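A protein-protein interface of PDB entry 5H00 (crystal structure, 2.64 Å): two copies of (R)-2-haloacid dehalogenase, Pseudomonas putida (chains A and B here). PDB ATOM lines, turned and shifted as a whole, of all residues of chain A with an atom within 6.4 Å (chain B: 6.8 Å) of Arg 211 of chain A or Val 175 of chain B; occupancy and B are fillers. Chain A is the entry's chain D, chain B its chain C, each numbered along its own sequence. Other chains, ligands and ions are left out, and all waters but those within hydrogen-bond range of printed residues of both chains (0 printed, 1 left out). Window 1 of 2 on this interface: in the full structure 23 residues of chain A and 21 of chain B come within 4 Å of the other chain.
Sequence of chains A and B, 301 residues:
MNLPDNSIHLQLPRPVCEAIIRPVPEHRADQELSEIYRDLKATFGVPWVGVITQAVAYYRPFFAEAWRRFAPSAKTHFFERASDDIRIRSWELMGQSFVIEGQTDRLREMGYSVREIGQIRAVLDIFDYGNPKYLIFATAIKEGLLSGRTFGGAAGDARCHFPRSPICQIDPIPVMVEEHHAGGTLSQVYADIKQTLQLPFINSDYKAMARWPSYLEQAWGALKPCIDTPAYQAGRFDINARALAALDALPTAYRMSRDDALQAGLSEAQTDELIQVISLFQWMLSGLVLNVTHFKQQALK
The guanidinium group of Arg 211 of chain B lies within hydrogen-bond range of the backbone carbonyl oxygen of Met 176 of chain A. The backbone carbonyl oxygen (O) of His 181 of chain B lies close to the backbone nitrogen (N) of Pro 213 of chain A (3.4 Å).
The backbone carbonyl oxygen of Val 177 of chain A is in hydrogen-bond range of the side-chain hydroxyl of Tyr 190 of chain A (2.7 Å). A ring nitrogen (ND1) of His 181 of chain B sits at hydrogen-bond distance from the backbone carbonyl oxygen (O) of Met 176 of chain B. The backbone NH of Val 177 of chain A lies within hydrogen-bond range of the backbone carbonyl oxygen of Lys 207 of chain A (3.0 Å). The backbone NH (N) of Glu 178 of chain B lies within hydrogen-bond range of a ring nitrogen (ND1) of His 181 of chain B, at 3.1 Å.
Among the printed residues, pairs that only touch across the chains: Arg 211 of chain A with Val 175 of chain B (3.6 Å), Trp 212 of chain A with His 181 of chain B (3.7 Å), Val 177 of chain A with Arg 211 of chain B (3.7 Å) and Val 175 of chain A with Arg 211 of chain B (3.8 Å).
Of chain A, only Arg 211 (3.6 Å) comes within 4 Å of Val 175 of chain B. Printed residues of chain B within 4 Å of Trp 212 of chain A: His 181. Printed residues of chain B within 4 Å of Pro 213 of chain A: His 181. Printed residues of chain B within 4 Å of Val 175 of chain A: Arg 211 (3.8 Å).
Hydrophobic or aromatic side chains of chain A that line the printed part of chain B: Val 175, Trp 212 and Pro 213. Among the printed residues, 6 pairs touch across the chains.
Val 175 of chain A touches Arg 211 of chain B, and with the chains exchanged Arg 211 of chain A touches Val 175 of chain B. Met 176 of chain A touches Arg 211 of chain B, but with the chains exchanged Arg 211 of chain A does not touch Met 176 of chain B (4.5 Å). Val 177 of chain A touches Arg 211 of chain B, but with the chains exchanged Arg 211 of chain A does not touch Val 177 of chain B (4.4 Å).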
ATOM      1  N   GLN A 119     -27.768   8.856  18.464  1.00  0.00           N
ATOM      2  CA  GLN A 119     -27.987   8.317  17.145  1.00  0.00           C
ATOM      3  C   GLN A 119     -27.261   6.986  17.029  1.00  0.00           C
ATOM      4  O   GLN A 119     -27.793   6.021  16.483  1.00  0.00           O
ATOM      5  CB  GLN A 119     -27.524   9.306  16.081  1.00  0.00           C
ATOM      6  CG  GLN A 119     -28.471  10.476  15.893  1.00  0.00           C
ATOM      7  CD  GLN A 119     -27.911  11.559  15.001  1.00  0.00           C
ATOM      8  OE1 GLN A 119     -26.867  11.404  14.379  1.00  0.00           O
ATOM      9  NE2 GLN A 119     -28.600  12.676  14.953  1.00  0.00           N
ATOM     10  N   VAL A 123     -29.042   3.038  16.633  1.00  0.00           N
ATOM     11  CA  VAL A 123     -28.564   2.084  15.642  1.00  0.00           C
ATOM     12  C   VAL A 123     -28.240   0.728  16.255  1.00  0.00           C
ATOM     13  O   VAL A 123     -28.646  -0.305  15.736  1.00  0.00           O
ATOM     14  CB  VAL A 123     -27.314   2.621  14.919  1.00  0.00           C
ATOM     15  CG1 VAL A 123     -26.583   1.520  14.189  1.00  0.00           C
ATOM     16  CG2 VAL A 123     -27.687   3.723  13.949  1.00  0.00           C
ATOM     17  N   VAL A 175     -28.261   3.265   7.421  1.00  0.00           N
ATOM     18  CA  VAL A 175     -27.164   3.674   6.553  1.00  0.00           C
ATOM     19  C   VAL A 175     -25.962   2.751   6.727  1.00  0.00           C
ATOM     20  O   VAL A 175     -25.377   2.672   7.810  1.00  0.00           O
ATOM     21  CB  VAL A 175     -26.726   5.117   6.839  1.00  0.00           C
ATOM     22  CG1 VAL A 175     -25.457   5.436   6.089  1.00  0.00           C
ATOM     23  CG2 VAL A 175     -27.829   6.093   6.496  1.00  0.00           C
ATOM     24  N   MET A 176     -25.597   2.048   5.659  1.00  0.00           N
ATOM     25  CA  MET A 176     -24.531   1.066   5.734  1.00  0.00           C
ATOM     26  C   MET A 176     -23.434   1.429   4.762  1.00  0.00           C
ATOM     27  O   MET A 176     -23.690   1.717   3.613  1.00  0.00           O
ATOM     28  CB  MET A 176     -25.073  -0.339   5.458  1.00  0.00           C
ATOM     29  CG  MET A 176     -26.005  -0.851   6.557  1.00  0.00           C
ATOM     30  SD  MET A 176     -26.769  -2.465   6.282  1.00  0.00           S
ATOM     31  CE  MET A 176     -27.733  -2.159   4.830  1.00  0.00           C
ATOM     32  N   VAL A 177     -22.204   1.443   5.243  1.00  0.00           N
ATOM     33  CA  VAL A 177     -21.071   1.735   4.389  1.00  0.00           C
ATOM     34  C   VAL A 177     -20.553   0.428   3.812  1.00  0.00           C
ATOM     35  O   VAL A 177     -19.766  -0.275   4.434  1.00  0.00           O
ATOM     36  CB  VAL A 177     -19.953   2.466   5.153  1.00  0.00           C
ATOM     37  CG1 VAL A 177     -18.828   2.839   4.215  1.00  0.00           C
ATOM     38  CG2 VAL A 177     -20.510   3.696   5.852  1.00  0.00           C
ATOM     39  N   TYR A 190     -12.128  -3.299   8.041  1.00  0.00           N
ATOM     40  CA  TYR A 190     -12.962  -4.375   7.518  1.00  0.00           C
ATOM     41  C   TYR A 190     -12.165  -5.666   7.366  1.00  0.00           C
ATOM     42  O   TYR A 190     -12.637  -6.756   7.701  1.00  0.00           O
ATOM     43  CB  TYR A 190     -13.565  -3.980   6.170  1.00  0.00           C
ATOM     44  CG  TYR A 190     -14.774  -3.080   6.257  1.00  0.00           C
ATOM     45  CD1 TYR A 190     -15.374  -2.813   7.473  1.00  0.00           C
ATOM     46  CD2 TYR A 190     -15.323  -2.507   5.113  1.00  0.00           C
ATOM     47  CE1 TYR A 190     -16.481  -1.991   7.555  1.00  0.00           C
ATOM     48  CE2 TYR A 190     -16.437  -1.690   5.182  1.00  0.00           C
ATOM     49  CZ  TYR A 190     -17.011  -1.432   6.408  1.00  0.00           C
ATOM     50  OH  TYR A 190     -18.115  -0.620   6.504  1.00  0.00           O
ATOM     51  N   TYR A 206     -21.673  -3.742  11.492  1.00  0.00           N
ATOM     52  CA  TYR A 206     -20.415  -3.028  11.462  1.00  0.00           C
ATOM     53  C   TYR A 206     -20.456  -1.988  10.350  1.00  0.00           C
ATOM     54  O   TYR A 206     -19.898  -0.900  10.491  1.00  0.00           O
ATOM     55  CB  TYR A 206     -19.247  -3.991  11.272  1.00  0.00           C
ATOM     56  CG  TYR A 206     -19.296  -5.205  12.175  1.00  0.00           C
ATOM     57  CD1 TYR A 206     -19.525  -5.077  13.541  1.00  0.00           C
ATOM     58  CD2 TYR A 206     -19.129  -6.486  11.661  1.00  0.00           C
ATOM     59  CE1 TYR A 206     -19.576  -6.192  14.366  1.00  0.00           C
ATOM     60  CE2 TYR A 206     -19.186  -7.596  12.476  1.00  0.00           C
ATOM     61  CZ  TYR A 206     -19.406  -7.450  13.826  1.00  0.00           C
ATOM     62  OH  TYR A 206     -19.457  -8.562  14.642  1.00  0.00           O
ATOM     63  N   LYS A 207     -21.106  -2.335   9.243  1.00  0.00           N
ATOM     64  CA  LYS A 207     -21.285  -1.407   8.146  1.00  0.00           C
ATOM     65  C   LYS A 207     -22.124  -0.219   8.613  1.00  0.00           C
ATOM     66  O   LYS A 207     -21.902   0.925   8.198  1.00  0.00           O
ATOM     67  CB  LYS A 207     -21.952  -2.095   6.946  1.00  0.00           C
ATOM     68  CG  LYS A 207     -21.140  -3.208   6.282  1.00  0.00           C
ATOM     69  CD  LYS A 207     -21.795  -3.707   4.988  1.00  0.00           C
ATOM     70  CE  LYS A 207     -23.133  -4.384   5.271  1.00  0.00           C
ATOM     71  NZ  LYS A 207     -23.860  -4.823   4.056  1.00  0.00           N
ATOM     72  N   ALA A 208     -23.098  -0.503   9.471  1.00  0.00           N
ATOM     73  CA  ALA A 208     -23.955   0.541  10.006  1.00  0.00           C
ATOM     74  C   ALA A 208     -23.170   1.436  10.968  1.00  0.00           C
ATOM     75  O   ALA A 208     -23.330   2.643  10.971  1.00  0.00           O
ATOM     76  CB  ALA A 208     -25.159  -0.058  10.689  1.00  0.00           C
ATOM     77  N   MET A 209     -22.313   0.828  11.774  1.00  0.00           N
ATOM     78  CA  MET A 209     -21.447   1.566  12.676  1.00  0.00           C
ATOM     79  C   MET A 209     -20.410   2.366  11.915  1.00  0.00           C
ATOM     80  O   MET A 209     -19.950   3.393  12.391  1.00  0.00           O
ATOM     81  CB  MET A 209     -20.757   0.609  13.648  1.00  0.00           C
ATOM     82  CG  MET A 209     -21.716  -0.085  14.587  1.00  0.00           C
ATOM     83  SD  MET A 209     -21.031  -1.535  15.402  1.00  0.00           S
ATOM     84  CE  MET A 209     -19.640  -0.792  16.240  1.00  0.00           C
ATOM     85  N   ALA A 210     -20.052   1.891  10.729  1.00  0.00           N
ATOM     86  CA  ALA A 210     -19.009   2.521   9.942  1.00  0.00           C
ATOM     87  C   ALA A 210     -19.480   3.826   9.316  1.00  0.00           C
ATOM     88  O   ALA A 210     -18.706   4.510   8.664  1.00  0.00           O
ATOM     89  CB  ALA A 210     -18.521   1.586   8.882  1.00  0.00           C
ATOM     90  N   ARG A 211     -20.747   4.170   9.506  1.00  0.00           N
ATOM     91  CA  ARG A 211     -21.201   5.501   9.164  1.00  0.00           C
ATOM     92  C   ARG A 211     -20.450   6.559   9.992  1.00  0.00           C
ATOM     93  O   ARG A 211     -20.244   7.679   9.536  1.00  0.00           O
ATOM     94  CB  ARG A 211     -22.703   5.640   9.369  1.00  0.00           C
ATOM     95  CG  ARG A 211     -23.207   7.055   9.140  1.00  0.00           C
ATOM     96  CD  ARG A 211     -24.150   7.492  10.231  1.00  0.00           C
ATOM     97  NE  ARG A 211     -24.346   8.934  10.236  1.00  0.00           N
ATOM     98  CZ  ARG A 211     -25.520   9.531  10.468  1.00  0.00           C
ATOM     99  NH1 ARG A 211     -26.615   8.806  10.711  1.00  0.00           N
ATOM    100  NH2 ARG A 211     -25.601  10.864  10.451  1.00  0.00           N
ATOM    101  N   TRP A 212     -20.053   6.194  11.208  1.00  0.00           N
ATOM    102  CA  TRP A 212     -19.134   6.996  12.019  1.00  0.00           C
ATOM    103  C   TRP A 212     -17.838   6.220  12.184  1.00  0.00           C
ATOM    104  O   TRP A 212     -17.649   5.538  13.187  1.00  0.00           O
ATOM    105  CB  TRP A 212     -19.693   7.309  13.419  1.00  0.00           C
ATOM    106  CG  TRP A 212     -21.040   7.923  13.488  1.00  0.00           C
ATOM    107  CD1 TRP A 212     -21.332   9.243  13.472  1.00  0.00           C
ATOM    108  CD2 TRP A 212     -22.286   7.237  13.628  1.00  0.00           C
ATOM    109  NE1 TRP A 212     -22.683   9.431  13.576  1.00  0.00           N
ATOM    110  CE2 TRP A 212     -23.293   8.212  13.670  1.00  0.00           C
ATOM    111  CE3 TRP A 212     -22.649   5.891  13.687  1.00  0.00           C
ATOM    112  CZ2 TRP A 212     -24.638   7.889  13.784  1.00  0.00           C
ATOM    113  CZ3 TRP A 212     -23.987   5.573  13.798  1.00  0.00           C
ATOM    114  CH2 TRP A 212     -24.966   6.567  13.851  1.00  0.00           C
ATOM    115  N   PRO A 213     -16.935   6.326  11.214  1.00  0.00           N
ATOM    116  CA  PRO A 213     -15.707   5.528  11.204  1.00  0.00           C
ATOM    117  C   PRO A 213     -14.867   5.580  12.480  1.00  0.00           C
ATOM    118  O   PRO A 213     -14.332   4.552  12.869  1.00  0.00           O
ATOM    119  CB  PRO A 213     -14.931   6.124  10.027  1.00  0.00           C
ATOM    120  CG  PRO A 213     -15.986   6.576   9.102  1.00  0.00           C
ATOM    121  CD  PRO A 213     -17.063   7.137   9.994  1.00  0.00           C
ATOM    122  N   LEU A 216     -16.456   3.361  15.043  1.00  0.00           N
ATOM    123  CA  LEU A 216     -16.286   1.939  14.782  1.00  0.00           C
ATOM    124  C   LEU A 216     -14.902   1.473  15.226  1.00  0.00           C
ATOM    125  O   LEU A 216     -14.775   0.435  15.867  1.00  0.00           O
ATOM    126  CB  LEU A 216     -16.503   1.617  13.310  1.00  0.00           C
ATOM    127  CG  LEU A 216     -16.183   0.167  12.906  1.00  0.00           C
ATOM    128  CD1 LEU A 216     -17.087  -0.801  13.610  1.00  0.00           C
ATOM    129  CD2 LEU A 216     -16.248  -0.046  11.404  1.00  0.00           C
ATOM    130  N   VAL B 123     -28.579  13.639  -3.589  1.00  0.00           N
ATOM    131  CA  VAL B 123     -27.752  14.409  -2.676  1.00  0.00           C
ATOM    132  C   VAL B 123     -27.119  15.633  -3.341  1.00  0.00           C
ATOM    133  O   VAL B 123     -27.208  16.749  -2.834  1.00  0.00           O
ATOM    134  CB  VAL B 123     -26.651  13.529  -2.092  1.00  0.00           C
ATOM    135  CG1 VAL B 123     -25.673  14.347  -1.288  1.00  0.00           C
ATOM    136  CG2 VAL B 123     -27.266  12.460  -1.236  1.00  0.00           C
ATOM    137  N   PRO B 172     -34.842  14.779   5.538  1.00  0.00           N
ATOM    138  CA  PRO B 172     -34.077  14.877   6.778  1.00  0.00           C
ATOM    139  C   PRO B 172     -32.790  15.634   6.557  1.00  0.00           C
ATOM    140  O   PRO B 172     -32.518  16.053   5.445  1.00  0.00           O
ATOM    141  CB  PRO B 172     -33.799  13.420   7.112  1.00  0.00           C
ATOM    142  CG  PRO B 172     -33.617  12.785   5.744  1.00  0.00           C
ATOM    143  CD  PRO B 172     -34.467  13.579   4.768  1.00  0.00           C
ATOM    144  N   ILE B 173     -32.012  15.823   7.610  1.00  0.00           N
ATOM    145  CA  ILE B 173     -30.688  16.388   7.466  1.00  0.00           C
ATOM    146  C   ILE B 173     -29.885  15.358   6.688  1.00  0.00           C
ATOM    147  O   ILE B 173     -29.953  14.173   6.970  1.00  0.00           O
ATOM    148  CB  ILE B 173     -30.052  16.709   8.838  1.00  0.00           C
ATOM    149  CG1 ILE B 173     -30.966  17.638   9.632  1.00  0.00           C
ATOM    150  CG2 ILE B 173     -28.687  17.382   8.703  1.00  0.00           C
ATOM    151  CD1 ILE B 173     -30.403  18.037  10.998  1.00  0.00           C
ATOM    152  N   PRO B 174     -29.174  15.797   5.653  1.00  0.00           N
ATOM    153  CA  PRO B 174     -28.262  14.888   4.954  1.00  0.00           C
ATOM    154  C   PRO B 174     -27.292  14.163   5.897  1.00  0.00           C
ATOM    155  O   PRO B 174     -26.852  14.714   6.906  1.00  0.00           O
ATOM    156  CB  PRO B 174     -27.506  15.825   4.017  1.00  0.00           C
ATOM    157  CG  PRO B 174     -28.474  16.930   3.754  1.00  0.00           C
ATOM    158  CD  PRO B 174     -29.268  17.112   4.999  1.00  0.00           C
ATOM    159  N   VAL B 175     -26.974  12.922   5.570  1.00  0.00           N
ATOM    160  CA  VAL B 175     -25.961  12.198   6.311  1.00  0.00           C
ATOM    161  C   VAL B 175     -24.614  12.823   6.008  1.00  0.00           C
ATOM    162  O   VAL B 175     -24.177  12.853   4.862  1.00  0.00           O
ATOM    163  CB  VAL B 175     -25.944  10.712   5.946  1.00  0.00           C
ATOM    164  CG1 VAL B 175     -24.933   9.968   6.797  1.00  0.00           C
ATOM    165  CG2 VAL B 175     -27.324  10.122   6.110  1.00  0.00           C
ATOM    166  N   MET B 176     -23.958  13.355   7.030  1.00  0.00           N
ATOM    167  CA  MET B 176     -22.685  14.022   6.795  1.00  0.00           C
ATOM    168  C   MET B 176     -21.609  13.396   7.660  1.00  0.00           C
ATOM    169  O   MET B 176     -21.815  13.183   8.848  1.00  0.00           O
ATOM    170  CB  MET B 176     -22.799  15.529   7.058  1.00  0.00           C
ATOM    171  CG  MET B 176     -23.559  16.303   5.978  1.00  0.00           C
ATOM    172  SD  MET B 176     -23.855  18.061   6.318  1.00  0.00           S
ATOM    173  CE  MET B 176     -24.898  18.003   7.761  1.00  0.00           C
ATOM    174  N   VAL B 177     -20.473  13.081   7.051  1.00  0.00           N
ATOM    175  CA  VAL B 177     -19.359  12.512   7.792  1.00  0.00           C
ATOM    176  C   VAL B 177     -18.473  13.646   8.258  1.00  0.00           C
ATOM    177  O   VAL B 177     -17.624  14.142   7.514  1.00  0.00           O
ATOM    178  CB  VAL B 177     -18.530  11.507   6.954  1.00  0.00           C
ATOM    179  CG1 VAL B 177     -17.576  10.747   7.850  1.00  0.00           C
ATOM    180  CG2 VAL B 177     -19.440  10.537   6.215  1.00  0.00           C
ATOM    181  N   GLU B 178     -18.707  14.054   9.500  1.00  0.00           N
ATOM    182  CA  GLU B 178     -18.041  15.190  10.093  1.00  0.00           C
ATOM    183  C   GLU B 178     -16.593  14.859  10.334  1.00  0.00           C
ATOM    184  O   GLU B 178     -16.205  13.698  10.311  1.00  0.00           O
ATOM    185  CB  GLU B 178     -18.720  15.576  11.398  1.00  0.00           C
ATOM    186  CG  GLU B 178     -20.205  15.743  11.270  1.00  0.00           C
ATOM    187  CD  GLU B 178     -20.597  17.052  10.658  1.00  0.00           C
ATOM    188  OE1 GLU B 178     -19.718  17.917  10.506  1.00  0.00           O
ATOM    189  OE2 GLU B 178     -21.783  17.222  10.339  1.00  0.00           O
ATOM    190  N   HIS B 181     -15.970  12.301  12.788  1.00  0.00           N
ATOM    191  CA  HIS B 181     -16.410  10.975  12.382  1.00  0.00           C
ATOM    192  C   HIS B 181     -15.297  10.294  11.586  1.00  0.00           C
ATOM    193  O   HIS B 181     -15.066   9.101  11.716  1.00  0.00           O
ATOM    194  CB  HIS B 181     -17.687  11.051  11.552  1.00  0.00           C
ATOM    195  CG  HIS B 181     -18.821  11.746  12.239  1.00  0.00           C
ATOM    196  ND1 HIS B 181     -19.957  12.137  11.572  1.00  0.00           N
ATOM    197  CD2 HIS B 181     -18.991  12.115  13.526  1.00  0.00           C
ATOM    198  CE1 HIS B 181     -20.786  12.716  12.423  1.00  0.00           C
ATOM    199  NE2 HIS B 181     -20.222  12.721  13.614  1.00  0.00           N
ATOM    200  N   ALA B 182     -14.593  11.089  10.787  1.00  0.00           N
ATOM    201  CA  ALA B 182     -13.594  10.610   9.838  1.00  0.00           C
ATOM    202  C   ALA B 182     -12.525   9.686  10.400  1.00  0.00           C
ATOM    203  O   ALA B 182     -12.053   9.858  11.517  1.00  0.00           O
ATOM    204  CB  ALA B 182     -12.921  11.791   9.187  1.00  0.00           C
ATOM    205  N   SER B 204     -20.416  21.165   3.943  1.00  0.00           N
ATOM    206  CA  SER B 204     -21.453  20.145   4.028  1.00  0.00           C
ATOM    207  C   SER B 204     -21.433  19.164   2.869  1.00  0.00           C
ATOM    208  O   SER B 204     -21.419  17.964   3.072  1.00  0.00           O
ATOM    209  CB  SER B 204     -22.821  20.804   4.099  1.00  0.00           C
ATOM    210  OG  SER B 204     -22.862  21.745   5.143  1.00  0.00           O
ATOM    211  N   LYS B 207     -18.881  16.571   2.801  1.00  0.00           N
ATOM    212  CA  LYS B 207     -19.199  15.692   3.914  1.00  0.00           C
ATOM    213  C   LYS B 207     -20.362  14.763   3.567  1.00  0.00           C
ATOM    214  O   LYS B 207     -20.429  13.636   4.037  1.00  0.00           O
ATOM    215  CB  LYS B 207     -19.531  16.503   5.160  1.00  0.00           C
ATOM    216  CG  LYS B 207     -18.399  17.383   5.648  1.00  0.00           C
ATOM    217  CD  LYS B 207     -18.647  17.985   7.037  1.00  0.00           C
ATOM    218  CE  LYS B 207     -19.740  19.030   7.030  1.00  0.00           C
ATOM    219  NZ  LYS B 207     -19.853  19.763   8.325  1.00  0.00           N
ATOM    220  N   ALA B 208     -21.280  15.239   2.739  1.00  0.00           N
ATOM    221  CA  ALA B 208     -22.418  14.428   2.336  1.00  0.00           C
ATOM    222  C   ALA B 208     -21.998  13.406   1.273  1.00  0.00           C
ATOM    223  O   ALA B 208     -22.500  12.288   1.225  1.00  0.00           O
ATOM    224  CB  ALA B 208     -23.544  15.312   1.830  1.00  0.00           C
ATOM    225  N   MET B 209     -21.072  13.794   0.418  1.00  0.00           N
ATOM    226  CA  MET B 209     -20.492  12.862  -0.526  1.00  0.00           C
ATOM    227  C   MET B 209     -19.678  11.812   0.211  1.00  0.00           C
ATOM    228  O   MET B 209     -19.681  10.655  -0.178  1.00  0.00           O
ATOM    229  CB  MET B 209     -19.642  13.611  -1.552  1.00  0.00           C
ATOM    230  CG  MET B 209     -20.459  14.598  -2.355  1.00  0.00           C
ATOM    231  SD  MET B 209     -19.526  15.734  -3.374  1.00  0.00           S
ATOM    232  CE  MET B 209     -18.619  14.611  -4.422  1.00  0.00           C
ATOM    233  N   ALA B 210     -19.023  12.220   1.295  1.00  0.00           N
ATOM    234  CA  ALA B 210     -18.243  11.315   2.160  1.00  0.00           C
ATOM    235  C   ALA B 210     -19.005  10.119   2.740  1.00  0.00           C
ATOM    236  O   ALA B 210     -18.389   9.195   3.224  1.00  0.00           O
ATOM    237  CB  ALA B 210     -17.640  12.098   3.291  1.00  0.00           C
ATOM    238  N   ARG B 211     -20.331  10.152   2.713  1.00  0.00           N
ATOM    239  CA  ARG B 211     -21.153   8.985   3.027  1.00  0.00           C
ATOM    240  C   ARG B 211     -20.738   7.800   2.109  1.00  0.00           C
ATOM    241  O   ARG B 211     -20.772   6.648   2.519  1.00  0.00           O
ATOM    242  CB  ARG B 211     -22.641   9.389   2.913  1.00  0.00           C
ATOM    243  CG  ARG B 211     -23.680   8.417   2.308  1.00  0.00           C
ATOM    244  CD  ARG B 211     -23.645   7.099   2.962  1.00  0.00           C
ATOM    245  NE  ARG B 211     -24.553   6.104   2.418  1.00  0.00           N
ATOM    246  CZ  ARG B 211     -24.270   4.811   2.428  1.00  0.00           C
ATOM    247  NH1 ARG B 211     -23.087   4.409   2.853  1.00  0.00           N
ATOM    248  NH2 ARG B 211     -25.141   3.929   1.977  1.00  0.00           N
